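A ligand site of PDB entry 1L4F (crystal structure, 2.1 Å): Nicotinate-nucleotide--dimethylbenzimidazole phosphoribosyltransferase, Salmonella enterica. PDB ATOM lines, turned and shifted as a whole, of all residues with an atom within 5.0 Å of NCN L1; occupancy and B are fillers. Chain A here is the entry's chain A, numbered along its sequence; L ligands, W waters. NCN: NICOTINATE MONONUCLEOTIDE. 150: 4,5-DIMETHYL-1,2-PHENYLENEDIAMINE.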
ATOM      1  N   VAL A  77       2.215  21.951 -25.607  1.00  0.00           N
ATOM      2  CA  VAL A  77       2.244  22.162 -24.156  1.00  0.00           C
ATOM      3  C   VAL A  77       2.030  20.900 -23.309  1.00  0.00           C
ATOM      4  O   VAL A  77       2.100  20.956 -22.073  1.00  0.00           O
ATOM      5  CB  VAL A  77       1.175  23.212 -23.713  1.00  0.00           C
ATOM      6  CG1 VAL A  77       1.471  24.572 -24.340  1.00  0.00           C
ATOM      7  CG2 VAL A  77      -0.219  22.754 -24.104  1.00  0.00           C
ATOM      8  N   ALA A  78       1.777  19.764 -23.956  1.00  0.00           N
ATOM      9  CA  ALA A  78       1.555  18.497 -23.254  1.00  0.00           C
ATOM     10  C   ALA A  78       2.347  17.348 -23.885  1.00  0.00           C
ATOM     11  O   ALA A  78       2.350  17.173 -25.108  1.00  0.00           O
ATOM     12  CB  ALA A  78       0.065  18.146 -23.258  1.00  0.00           C
ATOM     13  N   GLU A 174     -11.389  15.652 -13.352  1.00  0.00           N
ATOM     14  CA  GLU A 174     -11.294  15.837 -14.795  1.00  0.00           C
ATOM     15  C   GLU A 174     -10.327  14.895 -15.472  1.00  0.00           C
ATOM     16  O   GLU A 174      -9.592  14.141 -14.831  1.00  0.00           O
ATOM     17  CB  GLU A 174     -10.887  17.285 -15.113  1.00  0.00           C
ATOM     18  CG  GLU A 174      -9.730  17.832 -14.269  1.00  0.00           C
ATOM     19  CD  GLU A 174      -8.512  16.926 -14.268  1.00  0.00           C
ATOM     20  OE1 GLU A 174      -7.885  16.746 -15.327  1.00  0.00           O
ATOM     21  OE2 GLU A 174      -8.179  16.376 -13.195  1.00  0.00           O
ATOM     22  N   LEU A 175     -10.343  14.950 -16.806  1.00  0.00           N
ATOM     23  CA  LEU A 175      -9.473  14.136 -17.636  1.00  0.00           C
ATOM     24  C   LEU A 175      -9.391  14.850 -18.986  1.00  0.00           C
ATOM     25  O   LEU A 175     -10.391  14.963 -19.700  1.00  0.00           O
ATOM     26  CB  LEU A 175     -10.054  12.742 -17.818  1.00  0.00           C
ATOM     27  CG  LEU A 175      -9.236  11.766 -18.676  1.00  0.00           C
ATOM     28  CD1 LEU A 175      -7.853  11.572 -18.045  1.00  0.00           C
ATOM     29  CD2 LEU A 175      -9.967  10.436 -18.806  1.00  0.00           C
ATOM     30  N   GLY A 176      -8.206  15.341 -19.316  1.00  0.00           N
ATOM     31  CA  GLY A 176      -8.000  16.033 -20.575  1.00  0.00           C
ATOM     32  C   GLY A 176      -6.553  16.433 -20.763  1.00  0.00           C
ATOM     33  O   GLY A 176      -6.027  17.280 -20.036  1.00  0.00           O
ATOM     34  N   MET A 177      -5.895  15.822 -21.741  1.00  0.00           N
ATOM     35  CA  MET A 177      -4.496  16.121 -22.027  1.00  0.00           C
ATOM     36  C   MET A 177      -4.347  17.604 -22.353  1.00  0.00           C
ATOM     37  O   MET A 177      -5.126  18.155 -23.138  1.00  0.00           O
ATOM     38  CB  MET A 177      -3.997  15.270 -23.209  1.00  0.00           C
ATOM     39  CG  MET A 177      -4.207  13.774 -23.049  1.00  0.00           C
ATOM     40  SD  MET A 177      -3.488  13.083 -21.533  1.00  0.00           S
ATOM     41  CE  MET A 177      -4.925  13.017 -20.464  1.00  0.00           C
ATOM     42  N   ALA A 178      -3.365  18.239 -21.724  1.00  0.00           N
ATOM     43  CA  ALA A 178      -3.069  19.656 -21.896  1.00  0.00           C
ATOM     44  C   ALA A 178      -3.960  20.601 -21.089  1.00  0.00           C
ATOM     45  O   ALA A 178      -3.815  21.831 -21.203  1.00  0.00           O
ATOM     46  CB  ALA A 178      -3.137  20.046 -23.394  1.00  0.00           C
ATOM     47  N   ASN A 179      -4.852  20.079 -20.249  1.00  0.00           N
ATOM     48  CA  ASN A 179      -5.719  20.993 -19.506  1.00  0.00           C
ATOM     49  C   ASN A 179      -5.069  21.867 -18.415  1.00  0.00           C
ATOM     50  O   ASN A 179      -5.709  22.799 -17.926  1.00  0.00           O
ATOM     51  CB  ASN A 179      -6.972  20.274 -18.950  1.00  0.00           C
ATOM     52  CG  ASN A 179      -6.657  19.194 -17.925  1.00  0.00           C
ATOM     53  OD1 ASN A 179      -5.600  19.177 -17.317  1.00  0.00           O
ATOM     54  ND2 ASN A 179      -7.613  18.288 -17.722  1.00  0.00           N
ATOM     55  N   THR A 180      -3.816  21.613 -18.050  1.00  0.00           N
ATOM     56  CA  THR A 180      -3.184  22.463 -17.042  1.00  0.00           C
ATOM     57  C   THR A 180      -2.786  23.795 -17.685  1.00  0.00           C
ATOM     58  O   THR A 180      -2.406  24.744 -16.993  1.00  0.00           O
ATOM     59  CB  THR A 180      -1.927  21.822 -16.370  1.00  0.00           C
ATOM     60  OG1 THR A 180      -0.873  21.639 -17.339  1.00  0.00           O
ATOM     61  CG2 THR A 180      -2.277  20.491 -15.748  1.00  0.00           C
ATOM     62  N   THR A 181      -2.888  23.879 -19.011  1.00  0.00           N
ATOM     63  CA  THR A 181      -2.580  25.130 -19.691  1.00  0.00           C
ATOM     64  C   THR A 181      -3.745  26.105 -19.495  1.00  0.00           C
ATOM     65  O   THR A 181      -3.564  27.185 -18.958  1.00  0.00           O
ATOM     66  CB  THR A 181      -2.305  24.886 -21.188  1.00  0.00           C
ATOM     67  OG1 THR A 181      -1.086  24.146 -21.314  1.00  0.00           O
ATOM     68  CG2 THR A 181      -2.165  26.217 -21.926  1.00  0.00           C
ATOM     69  N   ILE A 201       4.468  21.942 -14.468  1.00  0.00           N
ATOM     70  CA  ILE A 201       4.876  20.918 -15.427  1.00  0.00           C
ATOM     71  C   ILE A 201       3.747  19.977 -15.854  1.00  0.00           C
ATOM     72  O   ILE A 201       3.956  19.079 -16.667  1.00  0.00           O
ATOM     73  CB  ILE A 201       6.020  20.025 -14.885  1.00  0.00           C
ATOM     74  CG1 ILE A 201       5.527  19.252 -13.665  1.00  0.00           C
ATOM     75  CG2 ILE A 201       7.218  20.889 -14.535  1.00  0.00           C
ATOM     76  CD1 ILE A 201       6.449  18.128 -13.239  1.00  0.00           C
ATOM     77  N   GLY A 202       2.553  20.186 -15.312  1.00  0.00           N
ATOM     78  CA  GLY A 202       1.435  19.324 -15.666  1.00  0.00           C
ATOM     79  C   GLY A 202       1.801  17.849 -15.533  1.00  0.00           C
ATOM     80  O   GLY A 202       2.326  17.429 -14.501  1.00  0.00           O
ATOM     81  N   ALA A 203       1.550  17.071 -16.574  1.00  0.00           N
ATOM     82  CA  ALA A 203       1.856  15.645 -16.543  1.00  0.00           C
ATOM     83  C   ALA A 203       3.283  15.369 -17.037  1.00  0.00           C
ATOM     84  O   ALA A 203       3.491  14.893 -18.161  1.00  0.00           O
ATOM     85  CB  ALA A 203       0.847  14.869 -17.383  1.00  0.00           C
ATOM     86  N   LYS A 213       5.253  26.871 -22.791  1.00  0.00           N
ATOM     87  CA  LYS A 213       3.952  26.820 -22.139  1.00  0.00           C
ATOM     88  C   LYS A 213       3.576  28.192 -21.568  1.00  0.00           C
ATOM     89  O   LYS A 213       2.418  28.609 -21.679  1.00  0.00           O
ATOM     90  CB  LYS A 213       3.967  25.757 -21.036  1.00  0.00           C
ATOM     91  CG  LYS A 213       2.603  25.439 -20.430  1.00  0.00           C
ATOM     92  CD  LYS A 213       2.684  24.189 -19.574  1.00  0.00           C
ATOM     93  CE  LYS A 213       1.404  23.930 -18.803  1.00  0.00           C
ATOM     94  NZ  LYS A 213       1.543  22.723 -17.942  1.00  0.00           N
ATOM     95  N   ASP A 263     -10.579  18.782  -5.923  1.00  0.00           N
ATOM     96  CA  ASP A 263      -9.506  17.816  -6.140  1.00  0.00           C
ATOM     97  C   ASP A 263      -8.168  18.576  -6.220  1.00  0.00           C
ATOM     98  O   ASP A 263      -7.716  19.098  -5.200  1.00  0.00           O
ATOM     99  CB  ASP A 263      -9.754  17.013  -7.446  1.00  0.00           C
ATOM    100  CG  ASP A 263      -8.676  15.942  -7.729  1.00  0.00           C
ATOM    101  OD1 ASP A 263      -8.087  15.385  -6.777  1.00  0.00           O
ATOM    102  OD2 ASP A 263      -8.440  15.648  -8.905  1.00  0.00           O
ATOM    103  N   GLY A 264      -7.582  18.658  -7.410  1.00  0.00           N
ATOM    104  CA  GLY A 264      -6.312  19.333  -7.563  1.00  0.00           C
ATOM    105  C   GLY A 264      -6.313  20.684  -8.262  1.00  0.00           C
ATOM    106  O   GLY A 264      -7.308  21.404  -8.271  1.00  0.00           O
ATOM    107  N   PHE A 265      -5.177  21.026  -8.879  1.00  0.00           N
ATOM    108  CA  PHE A 265      -5.018  22.303  -9.564  1.00  0.00           C
ATOM    109  C   PHE A 265      -6.140  22.654 -10.536  1.00  0.00           C
ATOM    110  O   PHE A 265      -6.618  23.784 -10.549  1.00  0.00           O
ATOM    111  CB  PHE A 265      -3.677  22.313 -10.316  1.00  0.00           C
ATOM    112  CG  PHE A 265      -3.336  23.663 -10.901  1.00  0.00           C
ATOM    113  CD1 PHE A 265      -3.322  23.860 -12.271  1.00  0.00           C
ATOM    114  CD2 PHE A 265      -3.037  24.735 -10.069  1.00  0.00           C
ATOM    115  CE1 PHE A 265      -3.027  25.106 -12.809  1.00  0.00           C
ATOM    116  CE2 PHE A 265      -2.737  25.990 -10.597  1.00  0.00           C
ATOM    117  CZ  PHE A 265      -2.743  26.177 -11.970  1.00  0.00           C
ATOM    118  N   LEU A 266      -6.561  21.688 -11.348  1.00  0.00           N
ATOM    119  CA  LEU A 266      -7.642  21.918 -12.293  1.00  0.00           C
ATOM    120  C   LEU A 266      -8.927  22.322 -11.571  1.00  0.00           C
ATOM    121  O   LEU A 266      -9.640  23.221 -12.012  1.00  0.00           O
ATOM    122  CB  LEU A 266      -7.898  20.673 -13.151  1.00  0.00           C
ATOM    123  CG  LEU A 266      -6.850  20.281 -14.204  1.00  0.00           C
ATOM    124  CD1 LEU A 266      -6.573  21.469 -15.099  1.00  0.00           C
ATOM    125  CD2 LEU A 266      -5.564  19.807 -13.540  1.00  0.00           C
ATOM    126  N   SER A 291      -2.240  20.157  -4.254  1.00  0.00           N
ATOM    127  CA  SER A 291      -1.604  19.783  -5.520  1.00  0.00           C
ATOM    128  C   SER A 291      -0.131  20.187  -5.662  1.00  0.00           C
ATOM    129  O   SER A 291       0.264  21.293  -5.280  1.00  0.00           O
ATOM    130  CB  SER A 291      -2.405  20.381  -6.688  1.00  0.00           C
ATOM    131  OG  SER A 291      -1.781  20.104  -7.930  1.00  0.00           O
ATOM    132  N   GLU A 293       1.257  20.944  -8.292  1.00  0.00           N
ATOM    133  CA  GLU A 293       1.390  21.868  -9.416  1.00  0.00           C
ATOM    134  C   GLU A 293       1.894  23.216  -8.871  1.00  0.00           C
ATOM    135  O   GLU A 293       1.483  23.646  -7.793  1.00  0.00           O
ATOM    136  CB  GLU A 293       0.028  22.009 -10.117  1.00  0.00           C
ATOM    137  CG  GLU A 293       0.000  22.894 -11.362  1.00  0.00           C
ATOM    138  CD  GLU A 293       0.517  22.233 -12.630  1.00  0.00           C
ATOM    139  OE1 GLU A 293       0.329  22.835 -13.700  1.00  0.00           O
ATOM    140  OE2 GLU A 293       1.089  21.119 -12.590  1.00  0.00           O
ATOM    141  N   MET A 313       0.357  15.028  -4.670  1.00  0.00           N
ATOM    142  CA  MET A 313      -0.324  14.394  -5.772  1.00  0.00           C
ATOM    143  C   MET A 313      -0.594  15.364  -6.915  1.00  0.00           C
ATOM    144  O   MET A 313      -0.798  16.569  -6.705  1.00  0.00           O
ATOM    145  CB  MET A 313      -1.623  13.749  -5.299  1.00  0.00           C
ATOM    146  CG  MET A 313      -1.407  12.471  -4.524  1.00  0.00           C
ATOM    147  SD  MET A 313      -2.854  11.947  -3.594  1.00  0.00           S
ATOM    148  CE  MET A 313      -4.042  11.607  -4.889  1.00  0.00           C
ATOM    149  N   ARG A 314      -0.584  14.829  -8.134  1.00  0.00           N
ATOM    150  CA  ARG A 314      -0.804  15.622  -9.333  1.00  0.00           C
ATOM    151  C   ARG A 314      -1.343  14.740 -10.461  1.00  0.00           C
ATOM    152  O   ARG A 314      -0.966  14.906 -11.615  1.00  0.00           O
ATOM    153  CB  ARG A 314       0.505  16.284  -9.755  1.00  0.00           C
ATOM    154  CG  ARG A 314       1.689  15.331  -9.919  1.00  0.00           C
ATOM    155  CD  ARG A 314       2.951  16.092 -10.284  1.00  0.00           C
ATOM    156  NE  ARG A 314       4.168  15.275 -10.224  1.00  0.00           N
ATOM    157  CZ  ARG A 314       4.542  14.391 -11.148  1.00  0.00           C
ATOM    158  NH1 ARG A 314       3.802  14.181 -12.224  1.00  0.00           N
ATOM    159  NH2 ARG A 314       5.689  13.728 -10.992  1.00  0.00           N
ATOM    160  N   LEU A 315      -2.210  13.788 -10.119  1.00  0.00           N
ATOM    161  CA  LEU A 315      -2.780  12.888 -11.116  1.00  0.00           C
ATOM    162  C   LEU A 315      -4.056  13.442 -11.738  1.00  0.00           C
ATOM    163  O   LEU A 315      -4.294  13.288 -12.933  1.00  0.00           O
ATOM    164  CB  LEU A 315      -3.097  11.532 -10.494  1.00  0.00           C
ATOM    165  CG  LEU A 315      -3.924  10.552 -11.338  1.00  0.00           C
ATOM    166  CD1 LEU A 315      -3.132  10.107 -12.571  1.00  0.00           C
ATOM    167  CD2 LEU A 315      -4.287   9.330 -10.497  1.00  0.00           C
ATOM    168  N   GLY A 316      -4.867  14.110 -10.915  1.00  0.00           N
ATOM    169  CA  GLY A 316      -6.138  14.632 -11.386  1.00  0.00           C
ATOM    170  C   GLY A 316      -7.174  13.535 -11.233  1.00  0.00           C
ATOM    171  O   GLY A 316      -7.077  12.727 -10.296  1.00  0.00           O
ATOM    172  N   GLU A 317      -8.150  13.494 -12.146  1.00  0.00           N
ATOM    173  CA  GLU A 317      -9.210  12.481 -12.156  1.00  0.00           C
ATOM    174  C   GLU A 317     -10.192  12.568 -10.992  1.00  0.00           C
ATOM    175  O   GLU A 317     -11.270  11.961 -11.026  1.00  0.00           O
ATOM    176  CB  GLU A 317      -8.604  11.088 -12.160  1.00  0.00           C
ATOM    177  CG  GLU A 317      -7.845  10.745 -13.414  1.00  0.00           C
ATOM    178  CD  GLU A 317      -7.288   9.352 -13.387  1.00  0.00           C
ATOM    179  OE1 GLU A 317      -7.824   8.517 -12.621  1.00  0.00           O
ATOM    180  OE2 GLU A 317      -6.335   9.079 -14.147  1.00  0.00           O
HETATM  181  P   NCN L   1      -1.028  18.201 -18.962  1.00  0.00           P
HETATM  182  O1P NCN L   1      -1.458  19.636 -19.073  1.00  0.00           O
HETATM  183  O2P NCN L   1       0.448  18.121 -18.979  1.00  0.00           O
HETATM  184  O3P NCN L   1      -1.626  17.340 -20.220  1.00  0.00           O
HETATM  185  O5' NCN L   1      -1.590  17.594 -17.616  1.00  0.00           O
HETATM  186  C5' NCN L   1      -3.011  17.591 -17.399  1.00  0.00           C
HETATM  187  C4' NCN L   1      -3.454  16.174 -17.259  1.00  0.00           C
HETATM  188  O4' NCN L   1      -2.721  15.567 -16.145  1.00  0.00           O
HETATM  189  C3' NCN L   1      -4.929  15.997 -16.976  1.00  0.00           C
HETATM  190  O3' NCN L   1      -5.542  14.913 -17.718  1.00  0.00           O
HETATM  191  C2' NCN L   1      -4.969  15.843 -15.422  1.00  0.00           C
HETATM  192  O2' NCN L   1      -5.891  14.756 -15.113  1.00  0.00           O
HETATM  193  C1' NCN L   1      -3.514  15.558 -14.989  1.00  0.00           C
HETATM  194  N1  NCN L   1      -2.895  16.494 -13.935  1.00  0.00           N
HETATM  195  C6  NCN L   1      -1.559  17.017 -14.093  1.00  0.00           C
HETATM  196  C5  NCN L   1      -1.134  17.850 -13.054  1.00  0.00           C
HETATM  197  C4  NCN L   1      -1.870  18.215 -11.900  1.00  0.00           C
HETATM  198  C3  NCN L   1      -3.199  17.624 -11.845  1.00  0.00           C
HETATM  199  C2  NCN L   1      -3.711  16.782 -12.839  1.00  0.00           C
HETATM  200  C7  NCN L   1      -3.837  18.114 -10.535  1.00  0.00           C
HETATM  201  O7  NCN L   1      -3.339  18.855  -9.694  1.00  0.00           O
HETATM  202  O8  NCN L   1      -5.074  17.603 -10.451  1.00  0.00           O
HETATM  203  N1  150 L   2      -5.079  11.022 -15.516  1.00  0.00           N
HETATM  204  N2  150 L   2      -3.627  13.163 -16.616  1.00  0.00           N
HETATM  205  C1  150 L   2      -4.027  10.751 -16.452  1.00  0.00           C
HETATM  206  C2  150 L   2      -3.317  11.815 -17.009  1.00  0.00           C
HETATM  207  C3  150 L   2      -2.349  11.595 -17.887  1.00  0.00           C
HETATM  208  C4  150 L   2      -2.041  10.324 -18.251  1.00  0.00           C
HETATM  209  C5  150 L   2      -2.735   9.261 -17.700  1.00  0.00           C
HETATM  210  C6  150 L   2      -3.739   9.495 -16.801  1.00  0.00           C
HETATM  211  C7  150 L   2      -0.929  10.058 -19.236  1.00  0.00           C
HETATM  212  C8  150 L   2      -2.383   7.856 -18.117  1.00  0.00           C
HETATM  213  O   HOH W   1       0.322  15.592 -21.167  1.00  0.00           O
HETATM  214  O   HOH W   2       2.523  16.783 -20.220  1.00  0.00           O
HETATM  215  O   HOH W   3      -0.585  21.563 -20.831  1.00  0.00           O
HETATM  216  O   HOH W   4      -7.792  18.909 -10.281  1.00  0.00           O
HETATM  217  O   HOH W   5      -5.641  15.964  -8.268  1.00  0.00           O
HETATM  218  O   HOH W   6       2.183  20.300 -19.457  1.00  0.00           O
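OG of Ser 291 is in hydrogen-bond range of O7 of NCN L1. O3' of NCN L1 is in hydrogen-bond range of N of Gly 176 (3.1 Å). An oxygen (O3') of NCN L1 is in hydrogen-bond range of the backbone carbonyl oxygen (O) of Gly 176, 3.3 Å away. The side-chain hydroxyl (OG1) of Thr 180 lies within hydrogen-bond range of an oxygen (O1P) of NCN L1, 2.7 Å away. N1 of 150 L2 lies within hydrogen-bond range of OE2 of Glu 317, 2.7 Å away. The side-chain carboxylate (OE1) of Glu 174 sits at hydrogen-bond distance from an oxygen (O2') of NCN L1 (2.8 Å). An oxygen (O2P) of NCN L1 is in hydrogen-bond range of the backbone NH (N) of Ala 203, at 2.8 Å. O1P of NCN L1 sits at hydrogen-bond distance from N of Thr 180, at 3.2 Å. The backbone NH (N) of Ala 178 lies within hydrogen-bond range of an oxygen (O3P) of NCN L1. N of Phe 265 lies within hydrogen-bond range of O7 of NCN L1, 3.0 Å away. The backbone carbonyl oxygen (O) of Leu 315 sits at hydrogen-bond distance from an oxygen (O2') of NCN L1, 3.1 Å away.
An oxygen (O4') of NCN L1 is in hydrogen-bond range of a nitrogen (N2) of 150 L2, 2.6 Å away.
The side-chain hydroxyl of Thr 180 lies within hydrogen-bond range of the side-chain amino group of Lys 213 (2.7 Å). The side-chain amide nitrogen (ND2) of Asn 179 lies within hydrogen-bond range of the side-chain carboxylate (OE1) of Glu 174 (2.9 Å). N of Glu 293 lies close to OG of Ser 291 (3.2 Å). The backbone NH (N) of Glu 317 lies within hydrogen-bond range of the side-chain carboxylate (OE2) of Glu 174 (3.1 Å). The backbone NH (N) of Gly 202 lies within hydrogen-bond range of the side-chain carboxylate (OE2) of Glu 293, 3.2 Å away. The backbone carbonyl oxygen (O) of Gly 176 lies close to the side-chain amide nitrogen (ND2) of Asn 179 (3.0 Å).
Water W3 lies within hydrogen-bond range of OG1 of Thr 181 (2.7 Å), O1P of NCN L1 (2.8 Å), O of Val 77 (3.0 Å) and O of Ala 178 (3.3 Å). Water W2 bridges O2P of NCN L1 (2.8 Å) and O of Ala 203 (3.0 Å). Water W5 lies within hydrogen-bond range of an oxygen (O8) of NCN L1 (2.8 Å), the side-chain carboxylate of Asp 263 (2.9 Å), the backbone NH of Gly 316 (3.3 Å) and the backbone NH of Gly 264 (3.4 Å). Water W6 lies within hydrogen-bond range of O of Val 77, O2P of NCN L1 and NZ of Lys 213. Water W4 lies within hydrogen-bond range of the backbone NH (N) of Gly 264 (2.9 Å), an oxygen (O8) of NCN L1 (3.0 Å) and the backbone NH (N) of Leu 266 (3.2 Å).
O of Arg 314 lies close to N1 of NCN L1, at 3.4 Å. Residues that only touch NCN L1: Asn 179, Gly 316, Met 177, Ala 78, Gly 264, Leu 266, Gly 202, Glu 317 and Glu 293. Hydrophobic or aromatic side chains that line NCN L1: Ala 78, Met 177, Ala 203, Phe 265 and Leu 266. Of the 25 residues printed, 18 come within 4 Å of NCN L1. The nearest printed residue that does not touch NCN L1 is Leu 175 (4.01 Å).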
